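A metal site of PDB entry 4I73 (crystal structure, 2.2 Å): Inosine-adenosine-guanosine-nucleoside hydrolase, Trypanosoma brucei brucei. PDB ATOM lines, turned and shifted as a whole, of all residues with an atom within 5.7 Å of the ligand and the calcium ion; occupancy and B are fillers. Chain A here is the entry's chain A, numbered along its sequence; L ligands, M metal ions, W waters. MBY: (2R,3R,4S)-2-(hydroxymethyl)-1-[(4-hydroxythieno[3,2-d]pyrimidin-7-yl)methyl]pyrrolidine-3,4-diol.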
ATOM      1  N   HIS A  12      21.354 -35.872 -29.636  1.00  0.00           N
ATOM      2  CA  HIS A  12      21.604 -34.564 -29.018  1.00  0.00           C
ATOM      3  C   HIS A  12      20.519 -33.541 -29.290  1.00  0.00           C
ATOM      4  O   HIS A  12      19.641 -33.776 -30.168  1.00  0.00           O
ATOM      5  CB  HIS A  12      22.932 -33.989 -29.481  1.00  0.00           C
ATOM      6  CG  HIS A  12      22.944 -33.532 -30.893  1.00  0.00           C
ATOM      7  ND1 HIS A  12      22.475 -32.303 -31.269  1.00  0.00           N
ATOM      8  CD2 HIS A  12      23.400 -34.133 -32.000  1.00  0.00           C
ATOM      9  CE1 HIS A  12      22.583 -32.178 -32.587  1.00  0.00           C
ATOM     10  NE2 HIS A  12      23.158 -33.279 -33.054  1.00  0.00           N
ATOM     11  N   ASP A  13      20.569 -32.423 -28.566  1.00  0.00           N
ATOM     12  CA  ASP A  13      19.605 -31.393 -28.803  1.00  0.00           C
ATOM     13  C   ASP A  13      20.198 -30.037 -29.155  1.00  0.00           C
ATOM     14  O   ASP A  13      19.625 -28.998 -28.813  1.00  0.00           O
ATOM     15  CB  ASP A  13      18.641 -31.302 -27.626  1.00  0.00           C
ATOM     16  CG  ASP A  13      19.285 -30.793 -26.385  1.00  0.00           C
ATOM     17  OD1 ASP A  13      20.545 -30.850 -26.261  1.00  0.00           O
ATOM     18  OD2 ASP A  13      18.469 -30.359 -25.514  1.00  0.00           O
ATOM     19  N   GLY A  14      21.363 -30.047 -29.797  1.00  0.00           N
ATOM     20  CA  GLY A  14      21.832 -28.860 -30.526  1.00  0.00           C
ATOM     21  C   GLY A  14      22.184 -27.566 -29.797  1.00  0.00           C
ATOM     22  O   GLY A  14      22.088 -26.467 -30.372  1.00  0.00           O
ATOM     23  N   ASN A  15      22.584 -27.624 -28.543  1.00  0.00           N
ATOM     24  CA  ASN A  15      23.178 -26.428 -27.946  1.00  0.00           C
ATOM     25  C   ASN A  15      24.715 -26.492 -28.129  1.00  0.00           C
ATOM     26  O   ASN A  15      25.216 -27.391 -28.776  1.00  0.00           O
ATOM     27  CB  ASN A  15      22.785 -26.263 -26.506  1.00  0.00           C
ATOM     28  CG  ASN A  15      22.577 -24.822 -26.111  1.00  0.00           C
ATOM     29  OD1 ASN A  15      23.512 -24.124 -25.636  1.00  0.00           O
ATOM     30  ND2 ASN A  15      21.344 -24.323 -26.332  1.00  0.00           N
ATOM     31  N   ASP A  17      27.383 -27.001 -26.201  1.00  0.00           N
ATOM     32  CA  ASP A  17      28.074 -28.156 -25.675  1.00  0.00           C
ATOM     33  C   ASP A  17      27.726 -29.451 -26.456  1.00  0.00           C
ATOM     34  O   ASP A  17      28.609 -30.269 -26.643  1.00  0.00           O
ATOM     35  CB  ASP A  17      27.841 -28.311 -24.178  1.00  0.00           C
ATOM     36  CG  ASP A  17      26.426 -28.700 -23.831  1.00  0.00           C
ATOM     37  OD1 ASP A  17      25.474 -28.317 -24.557  1.00  0.00           O
ATOM     38  OD2 ASP A  17      26.300 -29.424 -22.838  1.00  0.00           O
ATOM     39  N   ASP A  18      26.495 -29.607 -26.946  1.00  0.00           N
ATOM     40  CA  ASP A  18      26.154 -30.802 -27.737  1.00  0.00           C
ATOM     41  C   ASP A  18      27.125 -30.894 -28.902  1.00  0.00           C
ATOM     42  O   ASP A  18      27.587 -31.958 -29.239  1.00  0.00           O
ATOM     43  CB  ASP A  18      24.743 -30.764 -28.304  1.00  0.00           C
ATOM     44  CG  ASP A  18      23.678 -30.812 -27.232  1.00  0.00           C
ATOM     45  OD1 ASP A  18      23.126 -31.917 -26.973  1.00  0.00           O
ATOM     46  OD2 ASP A  18      23.385 -29.732 -26.654  1.00  0.00           O
ATOM     47  N   ASP A  43      16.770 -28.057 -26.700  1.00  0.00           N
ATOM     48  CA  ASP A  43      17.586 -26.890 -26.355  1.00  0.00           C
ATOM     49  C   ASP A  43      18.108 -26.209 -27.623  1.00  0.00           C
ATOM     50  O   ASP A  43      19.233 -25.649 -27.635  1.00  0.00           O
ATOM     51  CB  ASP A  43      18.754 -27.279 -25.494  1.00  0.00           C
ATOM     52  CG  ASP A  43      19.236 -26.172 -24.599  1.00  0.00           C
ATOM     53  OD1 ASP A  43      18.619 -25.077 -24.464  1.00  0.00           O
ATOM     54  OD2 ASP A  43      20.275 -26.383 -23.995  1.00  0.00           O
ATOM     55  N   PHE A  82      12.177 -25.703 -23.253  1.00  0.00           N
ATOM     56  CA  PHE A  82      13.331 -24.907 -22.873  1.00  0.00           C
ATOM     57  C   PHE A  82      13.093 -23.393 -23.073  1.00  0.00           C
ATOM     58  O   PHE A  82      12.337 -22.973 -23.962  1.00  0.00           O
ATOM     59  CB  PHE A  82      14.573 -25.317 -23.691  1.00  0.00           C
ATOM     60  CG  PHE A  82      15.315 -26.519 -23.143  1.00  0.00           C
ATOM     61  CD1 PHE A  82      16.268 -26.359 -22.154  1.00  0.00           C
ATOM     62  CD2 PHE A  82      15.140 -27.770 -23.666  1.00  0.00           C
ATOM     63  CE1 PHE A  82      16.984 -27.419 -21.664  1.00  0.00           C
ATOM     64  CE2 PHE A  82      15.863 -28.854 -23.176  1.00  0.00           C
ATOM     65  CZ  PHE A  82      16.807 -28.662 -22.194  1.00  0.00           C
ATOM     66  N   TRP A  86      17.901 -19.693 -24.755  1.00  0.00           N
ATOM     67  CA  TRP A  86      18.900 -20.733 -24.881  1.00  0.00           C
ATOM     68  C   TRP A  86      18.845 -21.487 -26.221  1.00  0.00           C
ATOM     69  O   TRP A  86      19.881 -21.876 -26.722  1.00  0.00           O
ATOM     70  CB  TRP A  86      18.743 -21.767 -23.774  1.00  0.00           C
ATOM     71  CG  TRP A  86      18.933 -21.269 -22.386  1.00  0.00           C
ATOM     72  CD1 TRP A  86      19.355 -20.052 -22.014  1.00  0.00           C
ATOM     73  CD2 TRP A  86      18.712 -22.009 -21.173  1.00  0.00           C
ATOM     74  NE1 TRP A  86      19.408 -19.959 -20.643  1.00  0.00           N
ATOM     75  CE2 TRP A  86      19.014 -21.146 -20.100  1.00  0.00           C
ATOM     76  CE3 TRP A  86      18.292 -23.313 -20.893  1.00  0.00           C
ATOM     77  CZ2 TRP A  86      18.905 -21.539 -18.772  1.00  0.00           C
ATOM     78  CZ3 TRP A  86      18.194 -23.716 -19.581  1.00  0.00           C
ATOM     79  CH2 TRP A  86      18.488 -22.822 -18.533  1.00  0.00           C
ATOM     80  N   THR A 140      22.685 -36.593 -25.332  1.00  0.00           N
ATOM     81  CA  THR A 140      23.046 -35.340 -24.687  1.00  0.00           C
ATOM     82  C   THR A 140      21.860 -34.345 -24.687  1.00  0.00           C
ATOM     83  O   THR A 140      22.011 -33.171 -24.266  1.00  0.00           O
ATOM     84  CB  THR A 140      24.279 -34.740 -25.331  1.00  0.00           C
ATOM     85  OG1 THR A 140      23.989 -34.464 -26.690  1.00  0.00           O
ATOM     86  CG2 THR A 140      25.452 -35.707 -25.229  1.00  0.00           C
ATOM     87  N   GLY A 141      20.718 -34.820 -25.177  1.00  0.00           N
ATOM     88  CA  GLY A 141      19.477 -34.135 -25.024  1.00  0.00           C
ATOM     89  C   GLY A 141      18.586 -34.978 -24.142  1.00  0.00           C
ATOM     90  O   GLY A 141      19.056 -35.865 -23.443  1.00  0.00           O
ATOM     91  N   MET A 167      23.801 -37.503 -20.449  1.00  0.00           N
ATOM     92  CA  MET A 167      23.892 -36.285 -19.680  1.00  0.00           C
ATOM     93  C   MET A 167      22.494 -35.969 -19.168  1.00  0.00           C
ATOM     94  O   MET A 167      21.561 -35.766 -19.944  1.00  0.00           O
ATOM     95  CB  MET A 167      24.437 -35.134 -20.525  1.00  0.00           C
ATOM     96  CG  MET A 167      24.960 -33.987 -19.675  1.00  0.00           C
ATOM     97  SD  MET A 167      23.578 -33.061 -19.018  1.00  0.00           S
ATOM     98  CE  MET A 167      23.985 -33.072 -17.274  1.00  0.00           C
ATOM     99  N   ASN A 176      19.030 -27.649 -11.988  1.00  0.00           N
ATOM    100  CA  ASN A 176      19.204 -26.392 -12.697  1.00  0.00           C
ATOM    101  C   ASN A 176      17.952 -25.849 -13.407  1.00  0.00           C
ATOM    102  O   ASN A 176      18.023 -24.881 -14.164  1.00  0.00           O
ATOM    103  CB  ASN A 176      20.426 -26.451 -13.611  1.00  0.00           C
ATOM    104  CG  ASN A 176      20.289 -27.456 -14.750  1.00  0.00           C
ATOM    105  OD1 ASN A 176      19.228 -28.046 -14.988  1.00  0.00           O
ATOM    106  ND2 ASN A 176      21.395 -27.621 -15.499  1.00  0.00           N
ATOM    107  N   GLU A 187      16.984 -31.334 -13.103  1.00  0.00           N
ATOM    108  CA  GLU A 187      17.920 -30.979 -14.178  1.00  0.00           C
ATOM    109  C   GLU A 187      17.141 -31.000 -15.503  1.00  0.00           C
ATOM    110  O   GLU A 187      16.208 -31.778 -15.674  1.00  0.00           O
ATOM    111  CB  GLU A 187      19.097 -31.965 -14.196  1.00  0.00           C
ATOM    112  CG  GLU A 187      20.115 -31.725 -15.325  1.00  0.00           C
ATOM    113  CD  GLU A 187      19.649 -32.266 -16.692  1.00  0.00           C
ATOM    114  OE1 GLU A 187      18.967 -33.312 -16.739  1.00  0.00           O
ATOM    115  OE2 GLU A 187      19.982 -31.636 -17.721  1.00  0.00           O
ATOM    116  N   TRP A 188      17.548 -30.116 -16.421  1.00  0.00           N
ATOM    117  CA  TRP A 188      16.725 -29.723 -17.580  1.00  0.00           C
ATOM    118  C   TRP A 188      16.415 -30.815 -18.593  1.00  0.00           C
ATOM    119  O   TRP A 188      15.300 -30.832 -19.128  1.00  0.00           O
ATOM    120  CB  TRP A 188      17.340 -28.505 -18.302  1.00  0.00           C
ATOM    121  CG  TRP A 188      16.686 -27.222 -17.957  1.00  0.00           C
ATOM    122  CD1 TRP A 188      17.164 -26.246 -17.109  1.00  0.00           C
ATOM    123  CD2 TRP A 188      15.384 -26.784 -18.376  1.00  0.00           C
ATOM    124  NE1 TRP A 188      16.234 -25.236 -16.978  1.00  0.00           N
ATOM    125  CE2 TRP A 188      15.148 -25.528 -17.779  1.00  0.00           C
ATOM    126  CE3 TRP A 188      14.431 -27.306 -19.258  1.00  0.00           C
ATOM    127  CZ2 TRP A 188      13.990 -24.786 -18.016  1.00  0.00           C
ATOM    128  CZ3 TRP A 188      13.275 -26.571 -19.489  1.00  0.00           C
ATOM    129  CH2 TRP A 188      13.051 -25.338 -18.844  1.00  0.00           C
ATOM    130  N   ASN A 189      17.402 -31.690 -18.899  1.00  0.00           N
ATOM    131  CA  ASN A 189      17.193 -32.783 -19.848  1.00  0.00           C
ATOM    132  C   ASN A 189      16.138 -33.807 -19.345  1.00  0.00           C
ATOM    133  O   ASN A 189      15.430 -34.420 -20.128  1.00  0.00           O
ATOM    134  CB  ASN A 189      18.499 -33.559 -20.167  1.00  0.00           C
ATOM    135  CG  ASN A 189      19.472 -32.788 -21.082  1.00  0.00           C
ATOM    136  OD1 ASN A 189      19.136 -31.786 -21.731  1.00  0.00           O
ATOM    137  ND2 ASN A 189      20.703 -33.263 -21.105  1.00  0.00           N
ATOM    138  N   LEU A 213      24.474 -33.559 -12.769  1.00  0.00           N
ATOM    139  CA  LEU A 213      25.076 -32.310 -12.353  1.00  0.00           C
ATOM    140  C   LEU A 213      26.205 -32.496 -11.311  1.00  0.00           C
ATOM    141  O   LEU A 213      27.112 -31.663 -11.242  1.00  0.00           O
ATOM    142  CB  LEU A 213      24.007 -31.339 -11.870  1.00  0.00           C
ATOM    143  CG  LEU A 213      22.976 -30.931 -12.961  1.00  0.00           C
ATOM    144  CD1 LEU A 213      21.983 -29.882 -12.407  1.00  0.00           C
ATOM    145  CD2 LEU A 213      23.707 -30.446 -14.261  1.00  0.00           C
ATOM    146  N   GLU A 251      28.555 -16.574 -18.550  1.00  0.00           N
ATOM    147  CA  GLU A 251      27.374 -17.000 -17.760  1.00  0.00           C
ATOM    148  C   GLU A 251      27.652 -17.161 -16.255  1.00  0.00           C
ATOM    149  O   GLU A 251      26.776 -16.816 -15.424  1.00  0.00           O
ATOM    150  CB  GLU A 251      26.758 -18.278 -18.321  1.00  0.00           C
ATOM    151  CG  GLU A 251      26.264 -18.174 -19.761  1.00  0.00           C
ATOM    152  CD  GLU A 251      24.981 -17.370 -19.915  1.00  0.00           C
ATOM    153  OE1 GLU A 251      24.404 -17.340 -21.016  1.00  0.00           O
ATOM    154  OE2 GLU A 251      24.504 -16.782 -18.913  1.00  0.00           O
ATOM    155  N   ARG A 255      25.321 -14.893 -13.959  1.00  0.00           N
ATOM    156  CA  ARG A 255      24.317 -15.661 -13.191  1.00  0.00           C
ATOM    157  C   ARG A 255      24.840 -16.122 -11.810  1.00  0.00           C
ATOM    158  O   ARG A 255      24.348 -17.111 -11.235  1.00  0.00           O
ATOM    159  CB  ARG A 255      23.802 -16.838 -14.016  1.00  0.00           C
ATOM    160  CG  ARG A 255      23.356 -16.453 -15.435  1.00  0.00           C
ATOM    161  CD  ARG A 255      22.671 -17.617 -16.190  1.00  0.00           C
ATOM    162  NE  ARG A 255      23.505 -18.829 -16.278  1.00  0.00           N
ATOM    163  CZ  ARG A 255      23.259 -19.873 -17.075  1.00  0.00           C
ATOM    164  NH1 ARG A 255      22.213 -19.876 -17.890  1.00  0.00           N
ATOM    165  NH2 ARG A 255      24.089 -20.913 -17.066  1.00  0.00           N
ATOM    166  N   ASP A 258      26.310 -19.663 -11.487  1.00  0.00           N
ATOM    167  CA  ASP A 258      25.573 -20.649 -12.281  1.00  0.00           C
ATOM    168  C   ASP A 258      26.135 -20.664 -13.705  1.00  0.00           C
ATOM    169  O   ASP A 258      25.573 -20.073 -14.624  1.00  0.00           O
ATOM    170  CB  ASP A 258      24.071 -20.349 -12.273  1.00  0.00           C
ATOM    171  CG  ASP A 258      23.265 -21.313 -13.146  1.00  0.00           C
ATOM    172  OD1 ASP A 258      23.605 -22.542 -13.148  1.00  0.00           O
ATOM    173  OD2 ASP A 258      22.305 -20.839 -13.824  1.00  0.00           O
ATOM    174  N   ALA A 259      27.267 -21.330 -13.866  1.00  0.00           N
ATOM    175  CA  ALA A 259      28.077 -21.247 -15.088  1.00  0.00           C
ATOM    176  C   ALA A 259      27.410 -21.982 -16.275  1.00  0.00           C
ATOM    177  O   ALA A 259      26.448 -22.745 -16.095  1.00  0.00           O
ATOM    178  CB  ALA A 259      29.517 -21.802 -14.823  1.00  0.00           C
ATOM    179  N   TYR A 260      27.884 -21.667 -17.491  1.00  0.00           N
ATOM    180  CA  TYR A 260      27.729 -22.566 -18.623  1.00  0.00           C
ATOM    181  C   TYR A 260      28.832 -23.593 -18.379  1.00  0.00           C
ATOM    182  O   TYR A 260      29.988 -23.232 -18.242  1.00  0.00           O
ATOM    183  CB  TYR A 260      27.914 -21.880 -19.987  1.00  0.00           C
ATOM    184  CG  TYR A 260      27.338 -22.673 -21.178  1.00  0.00           C
ATOM    185  CD1 TYR A 260      25.986 -22.513 -21.567  1.00  0.00           C
ATOM    186  CD2 TYR A 260      28.135 -23.557 -21.918  1.00  0.00           C
ATOM    187  CE1 TYR A 260      25.442 -23.232 -22.660  1.00  0.00           C
ATOM    188  CE2 TYR A 260      27.598 -24.299 -23.010  1.00  0.00           C
ATOM    189  CZ  TYR A 260      26.258 -24.134 -23.363  1.00  0.00           C
ATOM    190  OH  TYR A 260      25.782 -24.839 -24.430  1.00  0.00           O
ATOM    191  N   TRP A 263      28.894 -29.559 -20.026  1.00  0.00           N
ATOM    192  CA  TRP A 263      28.036 -30.669 -19.676  1.00  0.00           C
ATOM    193  C   TRP A 263      28.164 -31.850 -20.630  1.00  0.00           C
ATOM    194  O   TRP A 263      28.632 -32.933 -20.218  1.00  0.00           O
ATOM    195  CB  TRP A 263      26.563 -30.246 -19.671  1.00  0.00           C
ATOM    196  CG  TRP A 263      26.118 -29.158 -18.761  1.00  0.00           C
ATOM    197  CD1 TRP A 263      25.743 -29.284 -17.425  1.00  0.00           C
ATOM    198  CD2 TRP A 263      25.788 -27.824 -19.151  1.00  0.00           C
ATOM    199  NE1 TRP A 263      25.260 -28.067 -16.974  1.00  0.00           N
ATOM    200  CE2 TRP A 263      25.262 -27.170 -18.004  1.00  0.00           C
ATOM    201  CE3 TRP A 263      25.881 -27.105 -20.348  1.00  0.00           C
ATOM    202  CZ2 TRP A 263      24.860 -25.831 -18.028  1.00  0.00           C
ATOM    203  CZ3 TRP A 263      25.462 -25.762 -20.344  1.00  0.00           C
ATOM    204  CH2 TRP A 263      24.980 -25.154 -19.204  1.00  0.00           C
ATOM    205  N   ASP A 264      27.750 -31.650 -21.866  1.00  0.00           N
ATOM    206  CA  ASP A 264      27.668 -32.723 -22.831  1.00  0.00           C
ATOM    207  C   ASP A 264      29.037 -33.140 -23.312  1.00  0.00           C
ATOM    208  O   ASP A 264      29.199 -34.267 -23.791  1.00  0.00           O
ATOM    209  CB  ASP A 264      26.780 -32.352 -24.028  1.00  0.00           C
ATOM    210  CG  ASP A 264      25.336 -31.991 -23.625  1.00  0.00           C
ATOM    211  OD1 ASP A 264      24.927 -32.383 -22.523  1.00  0.00           O
ATOM    212  OD2 ASP A 264      24.608 -31.313 -24.401  1.00  0.00           O
HETATM  213  O6  MBY L   1      22.263 -22.096 -19.011  1.00  0.00           O
HETATM  214  C6  MBY L   1      21.954 -22.923 -19.860  1.00  0.00           C
HETATM  215  N1  MBY L   1      22.047 -22.650 -21.185  1.00  0.00           N
HETATM  216  C2  MBY L   1      21.669 -23.550 -22.134  1.00  0.00           C
HETATM  217  N3  MBY L   1      21.238 -24.755 -21.795  1.00  0.00           N
HETATM  218  C4  MBY L   1      21.122 -25.140 -20.519  1.00  0.00           C
HETATM  219  C5  MBY L   1      21.476 -24.254 -19.450  1.00  0.00           C
HETATM  220  C9  MBY L   1      20.668 -26.451 -19.946  1.00  0.00           C
HETATM  221  C8  MBY L   1      20.685 -26.436 -18.562  1.00  0.00           C
HETATM  222  S7  MBY L   1      21.260 -24.936 -17.926  1.00  0.00           S
HETATM  223  C7  MBY L   1      20.221 -27.658 -20.766  1.00  0.00           C
HETATM  224  N4' MBY L   1      21.339 -28.455 -21.357  1.00  0.00           N
HETATM  225  C4' MBY L   1      21.872 -29.639 -20.590  1.00  0.00           C
HETATM  226  C5' MBY L   1      22.226 -29.332 -19.134  1.00  0.00           C
HETATM  227  O5' MBY L   1      21.064 -29.464 -18.278  1.00  0.00           O
HETATM  228  C3' MBY L   1      23.119 -30.020 -21.374  1.00  0.00           C
HETATM  229  O3' MBY L   1      22.840 -31.110 -22.281  1.00  0.00           O
HETATM  230  C2' MBY L   1      23.482 -28.760 -22.206  1.00  0.00           C
HETATM  231  O2' MBY L   1      23.323 -29.040 -23.594  1.00  0.00           O
HETATM  232  C1' MBY L   1      22.515 -27.692 -21.831  1.00  0.00           C
HETATM  233 CA    CA M   1      22.284 -30.973 -24.774  1.00  0.00          CA
HETATM  234  O   HOH W   1      20.123 -30.010 -23.373  1.00  0.00           O
HETATM  235  O   HOH W   2      22.595 -21.742 -24.845  1.00  0.00           O
HETATM  236  O   HOH W   3      23.069 -20.576 -22.488  1.00  0.00           O
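Of the 24 residues printed, 4 come within 4 Å of the calcium ion.
Along chain A the residues within 4 Å of the calcium ion span positions 13 to 264.
The nearest printed residue that does not touch the calcium ion is Asp 17 (4.2 Å).
The guanidinium group (NH2) of Arg 255 lies within hydrogen-bond range of the backbone carbonyl oxygen (O) of Ala 259 (3.1 Å).
The side-chain carboxylate of Glu 251 is in salt-bridge range of the guanidinium group of Arg 255 (3.5 Å).
The backbone NH (N) of Asn 189 lies within hydrogen-bond range of the side-chain carboxylate (OE2) of Glu 187 (2.8 Å).
OD2 of Asp 18 lies close to N of Asn 15, 2.9 Å away.
O of Asp 43 sits at hydrogen-bond distance from ND2 of Asn 15, 2.8 Å away.
The side-chain amide nitrogen of Asn 189 is in hydrogen-bond range of the backbone carbonyl oxygen of Met 167, 2.9 Å away.
The side-chain amide oxygen (OD1) of Asn 176 is in hydrogen-bond range of the backbone NH (N) of Trp 188, at 3.0 Å.
The side-chain hydroxyl (OH) of Tyr 260 lies within hydrogen-bond range of the side-chain amide oxygen (OD1) of Asn 15 (2.7 Å).
Asn 15 touches the ligand.
Phe 82 touches the ligand.
Trp 86 touches the ligand (CZ3 to C5, 3.3 Å).
SD of Met 167 touches O3' of the ligand (3.9 Å).
CD1 of Trp 188 touches C8 of the ligand (3.8 Å).
Tyr 260 touches the ligand (CE1 to N1, 3.7 Å).
Trp 263 touches the ligand (CE3 to C2', 3.5 Å).
Hydrophobic or aromatic side chains within 4 Å of the ligand: Phe 82, Trp 86, Met 167, Trp 188, Tyr 260 and Trp 263.
Within 4 Å of the ligand: Asn 15, Asp 17, Asp 18, Asp 43, Phe 82, Trp 86, Thr 140, Met 167, Asn 176, Glu 187, Trp 188, Asn 189, Arg 255, Tyr 260, Trp 263 and Asp 264.
Water W1 bridges OD1 of Asn 189 (2.6 Å) and OD2 of Asp 13 (2.7 Å).
Water W2 lies within hydrogen-bond range of the side-chain amide oxygen of Asn 15 (2.7 Å) and the backbone carbonyl oxygen of Trp 86 (3.3 Å).
The calcium ion is bound by the backbone carbonyl oxygen (O) of Thr 140 (2.3 Å), the side-chain carboxylate (OD1) of Asp 13 (2.3 Å), the side-chain carboxylate (OD2) of Asp 264 (2.4 Å), an oxygen (O2') of the ligand (2.5 Å), the side-chain carboxylate (OD2) of Asp 18 (2.5 Å), the side-chain carboxylate (OD1) of Asp 18 (2.5 Å), an oxygen (O3') of the ligand (2.6 Å) and water W1 (2.7 Å).
The calcium ion has eight donor atoms within binding distance.
The side-chain carboxylate of Asp 17 lies close to an oxygen (O2') of the ligand, 2.5 Å away.
An oxygen (O6) of the ligand is in hydrogen-bond range of the guanidinium group (NH1) of Arg 255 (2.5 Å).
The side-chain carboxylate (OE2) of Glu 187 sits at hydrogen-bond distance from an oxygen (O5') of the ligand (2.5 Å).
The side-chain carboxylate (OD2) of Asp 43 lies within salt-bridge range of a nitrogen (N4') of the ligand (3.5 Å).
O3' of the ligand sits close to ND2 of Asn 189, 3.3 Å away.
The side-chain amide nitrogen (ND2) of Asn 176 lies within hydrogen-bond range of an oxygen (O5') of the ligand (3.4 Å).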
